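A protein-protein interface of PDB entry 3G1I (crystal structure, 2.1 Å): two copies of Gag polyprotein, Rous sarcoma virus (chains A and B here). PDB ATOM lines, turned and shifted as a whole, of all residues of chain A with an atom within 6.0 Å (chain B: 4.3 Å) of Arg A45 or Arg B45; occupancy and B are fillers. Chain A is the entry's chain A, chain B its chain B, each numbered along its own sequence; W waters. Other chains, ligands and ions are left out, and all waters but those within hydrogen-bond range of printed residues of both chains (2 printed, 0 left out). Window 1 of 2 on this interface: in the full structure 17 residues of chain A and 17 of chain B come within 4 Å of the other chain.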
ATOM      1  N   ILE A  40       1.745  22.319 -18.377  1.00  0.00           N
ATOM      2  CA  ILE A  40       0.320  22.582 -18.064  1.00  0.00           C
ATOM      3  C   ILE A  40      -0.365  21.288 -17.549  1.00  0.00           C
ATOM      4  O   ILE A  40      -0.994  21.296 -16.524  1.00  0.00           O
ATOM      5  CB  ILE A  40      -0.447  23.149 -19.305  1.00  0.00           C
ATOM      6  CG1 ILE A  40      -0.056  24.624 -19.570  1.00  0.00           C
ATOM      7  CG2 ILE A  40      -1.961  23.053 -19.094  1.00  0.00           C
ATOM      8  CD1 ILE A  40      -0.316  25.107 -21.007  1.00  0.00           C
ATOM      9  N   ILE A  41      -0.220  20.183 -18.264  1.00  0.00           N
ATOM     10  CA  ILE A  41      -0.842  18.913 -17.857  1.00  0.00           C
ATOM     11  C   ILE A  41      -0.337  18.436 -16.500  1.00  0.00           C
ATOM     12  O   ILE A  41      -1.127  17.993 -15.666  1.00  0.00           O
ATOM     13  CB  ILE A  41      -0.669  17.849 -18.954  1.00  0.00           C
ATOM     14  CG1 ILE A  41      -1.520  18.247 -20.164  1.00  0.00           C
ATOM     15  CG2 ILE A  41      -1.095  16.455 -18.457  1.00  0.00           C
ATOM     16  CD1 ILE A  41      -0.854  17.910 -21.463  1.00  0.00           C
ATOM     17  N   ASP A  42       0.968  18.594 -16.245  1.00  0.00           N
ATOM     18  CA  ASP A  42       1.517  18.287 -14.913  1.00  0.00           C
ATOM     19  C   ASP A  42       0.850  19.091 -13.807  1.00  0.00           C
ATOM     20  O   ASP A  42       0.518  18.544 -12.734  1.00  0.00           O
ATOM     21  CB  ASP A  42       3.045  18.518 -14.860  1.00  0.00           C
ATOM     22  CG  ASP A  42       3.640  18.100 -13.525  1.00  0.00           C
ATOM     23  OD1 ASP A  42       3.715  16.887 -13.284  1.00  0.00           O
ATOM     24  OD2 ASP A  42       4.024  18.969 -12.711  1.00  0.00           O
ATOM     25  N   CYS A  43       0.664  20.392 -14.040  1.00  0.00           N
ATOM     26  CA  CYS A  43      -0.025  21.233 -13.067  1.00  0.00           C
ATOM     27  C   CYS A  43      -1.507  20.769 -12.912  1.00  0.00           C
ATOM     28  O   CYS A  43      -1.991  20.680 -11.795  1.00  0.00           O
ATOM     29  CB  CYS A  43       0.037  22.718 -13.468  1.00  0.00           C
ATOM     30  SG  CYS A  43       1.775  23.485 -13.558  1.00  0.00           S
ATOM     31  N   PHE A  44      -2.212  20.513 -14.025  1.00  0.00           N
ATOM     32  CA  PHE A  44      -3.575  19.922 -13.921  1.00  0.00           C
ATOM     33  C   PHE A  44      -3.588  18.687 -12.967  1.00  0.00           C
ATOM     34  O   PHE A  44      -4.422  18.609 -12.086  1.00  0.00           O
ATOM     35  CB  PHE A  44      -4.124  19.514 -15.295  1.00  0.00           C
ATOM     36  CG  PHE A  44      -4.487  20.682 -16.219  1.00  0.00           C
ATOM     37  CD1 PHE A  44      -4.519  21.995 -15.776  1.00  0.00           C
ATOM     38  CD2 PHE A  44      -4.888  20.422 -17.526  1.00  0.00           C
ATOM     39  CE1 PHE A  44      -4.854  23.034 -16.653  1.00  0.00           C
ATOM     40  CE2 PHE A  44      -5.243  21.445 -18.387  1.00  0.00           C
ATOM     41  CZ  PHE A  44      -5.235  22.747 -17.954  1.00  0.00           C
ATOM     42  N   ARG A  45      -2.655  17.751 -13.150  1.00  0.00           N
ATOM     43  CA  ARG A  45      -2.605  16.494 -12.374  1.00  0.00           C
ATOM     44  C   ARG A  45      -2.286  16.690 -10.900  1.00  0.00           C
ATOM     45  O   ARG A  45      -2.786  15.945 -10.036  1.00  0.00           O
ATOM     46  CB  ARG A  45      -1.581  15.520 -12.950  1.00  0.00           C
ATOM     47  CG  ARG A  45      -1.994  14.929 -14.283  1.00  0.00           C
ATOM     48  CD  ARG A  45      -1.018  13.822 -14.792  1.00  0.00           C
ATOM     49  NE  ARG A  45      -1.562  13.264 -16.033  1.00  0.00           N
ATOM     50  CZ  ARG A  45      -2.479  12.299 -16.039  1.00  0.00           C
ATOM     51  NH1 ARG A  45      -2.874  11.771 -14.882  1.00  0.00           N
ATOM     52  NH2 ARG A  45      -2.991  11.854 -17.182  1.00  0.00           N
ATOM     53  N   GLN A  46      -1.462  17.697 -10.617  1.00  0.00           N
ATOM     54  CA  GLN A  46      -0.913  17.904  -9.293  1.00  0.00           C
ATOM     55  C   GLN A  46      -1.569  19.020  -8.513  1.00  0.00           C
ATOM     56  O   GLN A  46      -1.602  18.959  -7.304  1.00  0.00           O
ATOM     57  CB  GLN A  46       0.603  18.221  -9.384  1.00  0.00           C
ATOM     58  CG  GLN A  46       1.516  17.076  -9.766  1.00  0.00           C
ATOM     59  CD  GLN A  46       2.978  17.391  -9.449  1.00  0.00           C
ATOM     60  OE1 GLN A  46       3.274  18.154  -8.530  1.00  0.00           O
ATOM     61  NE2 GLN A  46       3.898  16.792 -10.206  1.00  0.00           N
ATOM     62  N   LYS A  47      -2.045  20.068  -9.173  1.00  0.00           N
ATOM     63  CA  LYS A  47      -2.482  21.258  -8.429  1.00  0.00           C
ATOM     64  C   LYS A  47      -3.987  21.542  -8.464  1.00  0.00           C
ATOM     65  O   LYS A  47      -4.458  22.564  -7.927  1.00  0.00           O
ATOM     66  CB  LYS A  47      -1.680  22.479  -8.879  1.00  0.00           C
ATOM     67  CG  LYS A  47      -0.173  22.301  -8.725  1.00  0.00           C
ATOM     68  CD  LYS A  47       0.588  23.340  -9.504  1.00  0.00           C
ATOM     69  CE  LYS A  47       2.083  23.037  -9.539  1.00  0.00           C
ATOM     70  NZ  LYS A  47       2.845  24.220  -9.971  1.00  0.00           N
ATOM     71  N   SER A  48      -4.743  20.658  -9.106  1.00  0.00           N
ATOM     72  CA  SER A  48      -6.204  20.762  -9.138  1.00  0.00           C
ATOM     73  C   SER A  48      -6.777  20.210  -7.836  1.00  0.00           C
ATOM     74  O   SER A  48      -6.079  19.514  -7.111  1.00  0.00           O
ATOM     75  CB  SER A  48      -6.766  19.960 -10.312  1.00  0.00           C
ATOM     76  OG  SER A  48      -6.402  18.587 -10.216  1.00  0.00           O
ATOM     77  N   GLN A  53      -8.348  15.806  -9.473  1.00  0.00           N
ATOM     78  CA  GLN A  53      -7.133  15.009  -9.508  1.00  0.00           C
ATOM     79  C   GLN A  53      -7.479  13.562  -9.797  1.00  0.00           C
ATOM     80  O   GLN A  53      -6.782  12.909 -10.541  1.00  0.00           O
ATOM     81  CB  GLN A  53      -6.357  15.119  -8.191  1.00  0.00           C
ATOM     82  CG  GLN A  53      -5.620  16.433  -8.045  1.00  0.00           C
ATOM     83  CD  GLN A  53      -4.596  16.408  -6.906  1.00  0.00           C
ATOM     84  OE1 GLN A  53      -4.103  15.355  -6.523  1.00  0.00           O
ATOM     85  NE2 GLN A  53      -4.250  17.584  -6.391  1.00  0.00           N
ATOM     86  N   ILE A  56      -8.519  13.130 -13.603  1.00  0.00           N
ATOM     87  CA  ILE A  56      -7.354  13.157 -14.492  1.00  0.00           C
ATOM     88  C   ILE A  56      -6.419  11.936 -14.319  1.00  0.00           C
ATOM     89  O   ILE A  56      -5.839  11.431 -15.297  1.00  0.00           O
ATOM     90  CB  ILE A  56      -6.589  14.507 -14.313  1.00  0.00           C
ATOM     91  CG1 ILE A  56      -7.496  15.694 -14.700  1.00  0.00           C
ATOM     92  CG2 ILE A  56      -5.289  14.528 -15.168  1.00  0.00           C
ATOM     93  CD1 ILE A  56      -6.908  17.088 -14.342  1.00  0.00           C
ATOM     94  N   ARG A  57      -6.299  11.455 -13.073  1.00  0.00           N
ATOM     95  CA  ARG A  57      -5.485  10.275 -12.759  1.00  0.00           C
ATOM     96  C   ARG A  57      -5.702   9.120 -13.727  1.00  0.00           C
ATOM     97  O   ARG A  57      -4.737   8.570 -14.298  1.00  0.00           O
ATOM     98  CB  ARG A  57      -5.834   9.816 -11.339  1.00  0.00           C
ATOM     99  CG  ARG A  57      -5.126   8.539 -10.922  1.00  0.00           C
ATOM    100  CD  ARG A  57      -5.671   8.077  -9.566  1.00  0.00           C
ATOM    101  NE  ARG A  57      -5.070   6.804  -9.147  1.00  0.00           N
ATOM    102  CZ  ARG A  57      -5.496   6.070  -8.122  1.00  0.00           C
ATOM    103  NH1 ARG A  57      -6.561   6.444  -7.409  1.00  0.00           N
ATOM    104  NH2 ARG A  57      -4.854   4.943  -7.819  1.00  0.00           N
ATOM    105  N   THR A  58      -6.978   8.775 -13.943  1.00  0.00           N
ATOM    106  CA  THR A  58      -7.355   7.607 -14.762  1.00  0.00           C
ATOM    107  C   THR A  58      -7.756   7.951 -16.217  1.00  0.00           C
ATOM    108  O   THR A  58      -8.285   7.111 -16.947  1.00  0.00           O
ATOM    109  CB  THR A  58      -8.476   6.809 -14.071  1.00  0.00           C
ATOM    110  OG1 THR A  58      -9.476   7.723 -13.619  1.00  0.00           O
ATOM    111  CG2 THR A  58      -7.928   6.102 -12.829  1.00  0.00           C
ATOM    112  N   ALA A  59      -7.474   9.187 -16.643  1.00  0.00           N
ATOM    113  CA  ALA A  59      -7.673   9.581 -18.049  1.00  0.00           C
ATOM    114  C   ALA A  59      -6.876   8.681 -18.967  1.00  0.00           C
ATOM    115  O   ALA A  59      -5.799   8.202 -18.575  1.00  0.00           O
ATOM    116  CB  ALA A  59      -7.254  11.067 -18.271  1.00  0.00           C
ATOM    117  N   PRO A  60      -7.394   8.436 -20.199  1.00  0.00           N
ATOM    118  CA  PRO A  60      -6.656   7.695 -21.187  1.00  0.00           C
ATOM    119  C   PRO A  60      -5.290   8.328 -21.420  1.00  0.00           C
ATOM    120  O   PRO A  60      -5.150   9.554 -21.345  1.00  0.00           O
ATOM    121  CB  PRO A  60      -7.530   7.811 -22.444  1.00  0.00           C
ATOM    122  CG  PRO A  60      -8.904   7.929 -21.908  1.00  0.00           C
ATOM    123  CD  PRO A  60      -8.726   8.809 -20.694  1.00  0.00           C
ATOM    124  N   SER A  61      -4.304   7.482 -21.685  1.00  0.00           N
ATOM    125  CA  SER A  61      -2.916   7.910 -21.830  1.00  0.00           C
ATOM    126  C   SER A  61      -2.671   8.620 -23.182  1.00  0.00           C
ATOM    127  O   SER A  61      -1.581   9.177 -23.439  1.00  0.00           O
ATOM    128  CB  SER A  61      -2.031   6.680 -21.705  1.00  0.00           C
ATOM    129  OG  SER A  61      -2.378   5.761 -22.727  1.00  0.00           O
ATOM    130  N   LEU A  63      -4.431  11.232 -24.114  1.00  0.00           N
ATOM    131  CA  LEU A  63      -4.823  12.629 -24.000  1.00  0.00           C
ATOM    132  C   LEU A  63      -3.592  13.435 -23.575  1.00  0.00           C
ATOM    133  O   LEU A  63      -3.196  13.396 -22.427  1.00  0.00           O
ATOM    134  CB  LEU A  63      -6.008  12.813 -23.047  1.00  0.00           C
ATOM    135  CG  LEU A  63      -7.279  11.990 -23.293  1.00  0.00           C
ATOM    136  CD1 LEU A  63      -8.349  12.421 -22.333  1.00  0.00           C
ATOM    137  CD2 LEU A  63      -7.790  12.089 -24.719  1.00  0.00           C
ATOM    138  N   ILE A  69      -7.411  17.314 -22.207  1.00  0.00           N
ATOM    139  CA  ILE A  69      -7.677  16.991 -20.805  1.00  0.00           C
ATOM    140  C   ILE A  69      -8.847  17.810 -20.282  1.00  0.00           C
ATOM    141  O   ILE A  69      -9.668  17.318 -19.486  1.00  0.00           O
ATOM    142  CB  ILE A  69      -6.439  17.200 -19.926  1.00  0.00           C
ATOM    143  CG1 ILE A  69      -5.342  16.204 -20.317  1.00  0.00           C
ATOM    144  CG2 ILE A  69      -6.817  17.207 -18.413  1.00  0.00           C
ATOM    145  CD1 ILE A  69      -5.495  14.777 -19.715  1.00  0.00           C
ATOM    146  N   ILE B  41       7.747  12.868 -17.022  1.00  0.00           N
ATOM    147  CA  ILE B  41       6.531  12.197 -16.552  1.00  0.00           C
ATOM    148  C   ILE B  41       5.562  12.039 -17.717  1.00  0.00           C
ATOM    149  O   ILE B  41       5.020  10.959 -17.932  1.00  0.00           O
ATOM    150  CB  ILE B  41       5.868  12.958 -15.376  1.00  0.00           C
ATOM    151  CG1 ILE B  41       6.789  12.992 -14.158  1.00  0.00           C
ATOM    152  CG2 ILE B  41       4.531  12.300 -14.976  1.00  0.00           C
ATOM    153  CD1 ILE B  41       6.317  13.980 -13.064  1.00  0.00           C
ATOM    154  N   ASP B  42       5.394  13.099 -18.500  1.00  0.00           N
ATOM    155  CA  ASP B  42       4.586  13.033 -19.704  1.00  0.00           C
ATOM    156  C   ASP B  42       5.065  11.939 -20.671  1.00  0.00           C
ATOM    157  O   ASP B  42       4.251  11.154 -21.202  1.00  0.00           O
ATOM    158  CB  ASP B  42       4.595  14.379 -20.414  1.00  0.00           C
ATOM    159  CG  ASP B  42       3.702  14.390 -21.636  1.00  0.00           C
ATOM    160  OD1 ASP B  42       2.509  14.674 -21.467  1.00  0.00           O
ATOM    161  OD2 ASP B  42       4.181  14.105 -22.754  1.00  0.00           O
ATOM    162  N   CYS B  43       6.373  11.879 -20.918  1.00  0.00           N
ATOM    163  CA  CYS B  43       6.891  10.843 -21.785  1.00  0.00           C
ATOM    164  C   CYS B  43       6.636   9.442 -21.207  1.00  0.00           C
ATOM    165  O   CYS B  43       6.315   8.522 -21.969  1.00  0.00           O
ATOM    166  CB  CYS B  43       8.394  11.035 -22.014  1.00  0.00           C
ATOM    167  SG  CYS B  43       8.805  12.542 -22.920  1.00  0.00           S
ATOM    168  N   PHE B  44       6.821   9.280 -19.892  1.00  0.00           N
ATOM    169  CA  PHE B  44       6.455   8.013 -19.224  1.00  0.00           C
ATOM    170  C   PHE B  44       4.983   7.650 -19.460  1.00  0.00           C
ATOM    171  O   PHE B  44       4.664   6.528 -19.853  1.00  0.00           O
ATOM    172  CB  PHE B  44       6.679   8.085 -17.706  1.00  0.00           C
ATOM    173  CG  PHE B  44       8.108   7.979 -17.286  1.00  0.00           C
ATOM    174  CD1 PHE B  44       9.062   7.379 -18.110  1.00  0.00           C
ATOM    175  CD2 PHE B  44       8.508   8.453 -16.047  1.00  0.00           C
ATOM    176  CE1 PHE B  44      10.405   7.294 -17.701  1.00  0.00           C
ATOM    177  CE2 PHE B  44       9.842   8.367 -15.648  1.00  0.00           C
ATOM    178  CZ  PHE B  44      10.782   7.792 -16.481  1.00  0.00           C
ATOM    179  N   ARG B  45       4.099   8.616 -19.200  1.00  0.00           N
ATOM    180  CA  ARG B  45       2.656   8.379 -19.221  1.00  0.00           C
ATOM    181  C   ARG B  45       2.165   8.027 -20.611  1.00  0.00           C
ATOM    182  O   ARG B  45       1.223   7.246 -20.769  1.00  0.00           O
ATOM    183  CB  ARG B  45       1.920   9.605 -18.697  1.00  0.00           C
ATOM    184  CG  ARG B  45       2.085   9.783 -17.204  1.00  0.00           C
ATOM    185  CD  ARG B  45       1.280  10.985 -16.728  1.00  0.00           C
ATOM    186  NE  ARG B  45       1.362  11.101 -15.270  1.00  0.00           N
ATOM    187  CZ  ARG B  45       0.632  10.389 -14.417  1.00  0.00           C
ATOM    188  NH1 ARG B  45      -0.234   9.484 -14.858  1.00  0.00           N
ATOM    189  NH2 ARG B  45       0.780  10.579 -13.115  1.00  0.00           N
ATOM    190  N   GLN B  46       2.848   8.565 -21.616  1.00  0.00           N
ATOM    191  CA  GLN B  46       2.335   8.588 -22.979  1.00  0.00           C
ATOM    192  C   GLN B  46       3.152   7.769 -23.992  1.00  0.00           C
ATOM    193  O   GLN B  46       2.613   7.313 -25.022  1.00  0.00           O
ATOM    194  CB  GLN B  46       2.179  10.060 -23.427  1.00  0.00           C
ATOM    195  CG  GLN B  46       1.758  10.231 -24.862  1.00  0.00           C
ATOM    196  CD  GLN B  46       2.406  11.427 -25.543  1.00  0.00           C
ATOM    197  OE1 GLN B  46       2.783  12.417 -24.905  1.00  0.00           O
ATOM    198  NE2 GLN B  46       2.512  11.345 -26.854  1.00  0.00           N
ATOM    199  N   LYS B  47       4.433   7.559 -23.719  1.00  0.00           N
ATOM    200  CA  LYS B  47       5.329   6.978 -24.736  1.00  0.00           C
ATOM    201  C   LYS B  47       6.035   5.700 -24.283  1.00  0.00           C
ATOM    202  O   LYS B  47       6.836   5.130 -25.032  1.00  0.00           O
ATOM    203  CB  LYS B  47       6.327   8.028 -25.268  1.00  0.00           C
ATOM    204  CG  LYS B  47       5.629   9.144 -26.083  1.00  0.00           C
ATOM    205  CD  LYS B  47       6.626  10.093 -26.754  1.00  0.00           C
ATOM    206  N   GLN B  53       1.945   2.057 -20.063  1.00  0.00           N
ATOM    207  CA  GLN B  53       1.073   3.238 -20.009  1.00  0.00           C
ATOM    208  C   GLN B  53      -0.159   2.955 -19.138  1.00  0.00           C
ATOM    209  O   GLN B  53      -0.603   3.820 -18.370  1.00  0.00           O
ATOM    210  CB  GLN B  53       0.596   3.665 -21.393  1.00  0.00           C
ATOM    211  CG  GLN B  53       1.687   4.140 -22.336  1.00  0.00           C
ATOM    212  CD  GLN B  53       1.143   4.322 -23.731  1.00  0.00           C
ATOM    213  OE1 GLN B  53       1.694   3.805 -24.701  1.00  0.00           O
ATOM    214  NE2 GLN B  53       0.034   5.030 -23.835  1.00  0.00           N
ATOM    215  N   ILE B  56       0.689   2.884 -15.309  1.00  0.00           N
ATOM    216  CA  ILE B  56       0.855   4.261 -14.763  1.00  0.00           C
ATOM    217  C   ILE B  56      -0.484   4.988 -14.600  1.00  0.00           C
ATOM    218  O   ILE B  56      -0.703   5.739 -13.646  1.00  0.00           O
ATOM    219  CB  ILE B  56       1.835   5.087 -15.630  1.00  0.00           C
ATOM    220  CG1 ILE B  56       3.255   4.490 -15.512  1.00  0.00           C
ATOM    221  CG2 ILE B  56       1.862   6.572 -15.189  1.00  0.00           C
ATOM    222  CD1 ILE B  56       4.170   4.944 -16.574  1.00  0.00           C
HETATM  223  O   HOH W   1      -2.307   8.098 -13.199  1.00  0.00           O
HETATM  224  O   HOH W   2      -0.440   7.614 -25.609  1.00  0.00           O
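The side-chain hydroxyl (OG) of Ser A61 sits at hydrogen-bond distance from the side-chain amide nitrogen (NE2) of Gln B53, 2.8 Å away.
NH1 of Arg A45 lies close to NH1 of Arg B45.
Among the printed residues, pairs that only touch across the chains: Asp A42 with Ile B41 (3.9 Å), Ser A61 with Arg B45 (3.4 Å) and Ser A61 with Gln B46 (3.8 Å).
Of the 9 printed residues of chain B, 4 touch a printed residue of chain A.
Asp A42 touches Ile B41, but with the chains exchanged Ile A41 does not touch Asp B42 (4.7 Å).
Arg A45 touches its own counterpart, Arg B45.
Of the 5 pairs that touch across the chains among the printed residues, 1 has its exchanged pair printed and touching as well.
The side-chain carboxylate (OD2) of Asp B42 sits close to the side-chain amide oxygen (OE1) of Gln B46, at 3.1 Å.
The side-chain amide nitrogen (NE2) of Gln A46 sits at hydrogen-bond distance from the side-chain carboxylate (OD1) of Asp A42 (3.1 Å).
The guanidinium group (NH1) of Arg A45 is in hydrogen-bond range of the backbone carbonyl oxygen (O) of Ile A56 (3.0 Å).
Arg A45 touches just one residue of chain B: Arg B45.
Of chain A, only Arg A45 (3.5 Å) and Ser A61 (3.4 Å) come within 4 Å of Arg B45.
Printed residues of chain A within 4 Å of Ile B41: Asp A42 (3.9 Å).
Of the printed residues of chain A, Gln B53 touches Ser A61 (2.8 Å).
Printed residues of chain B within 4 Å of Asp A42: Ile B41.
Cys B43 touches none of the printed residues of chain A.
The nearest printed residue of chain A that does not touch Gln B53 is Pro A60 (6.7 Å).
Water W1 lies within hydrogen-bond range of O of Arg A57, O of Ile B56 and NH1 of Arg B45.
Water W2 lies within hydrogen-bond range of O of Ser A61 (2.9 Å), O of Gln B46 (3.1 Å) and NE2 of Gln B53 (3.2 Å).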
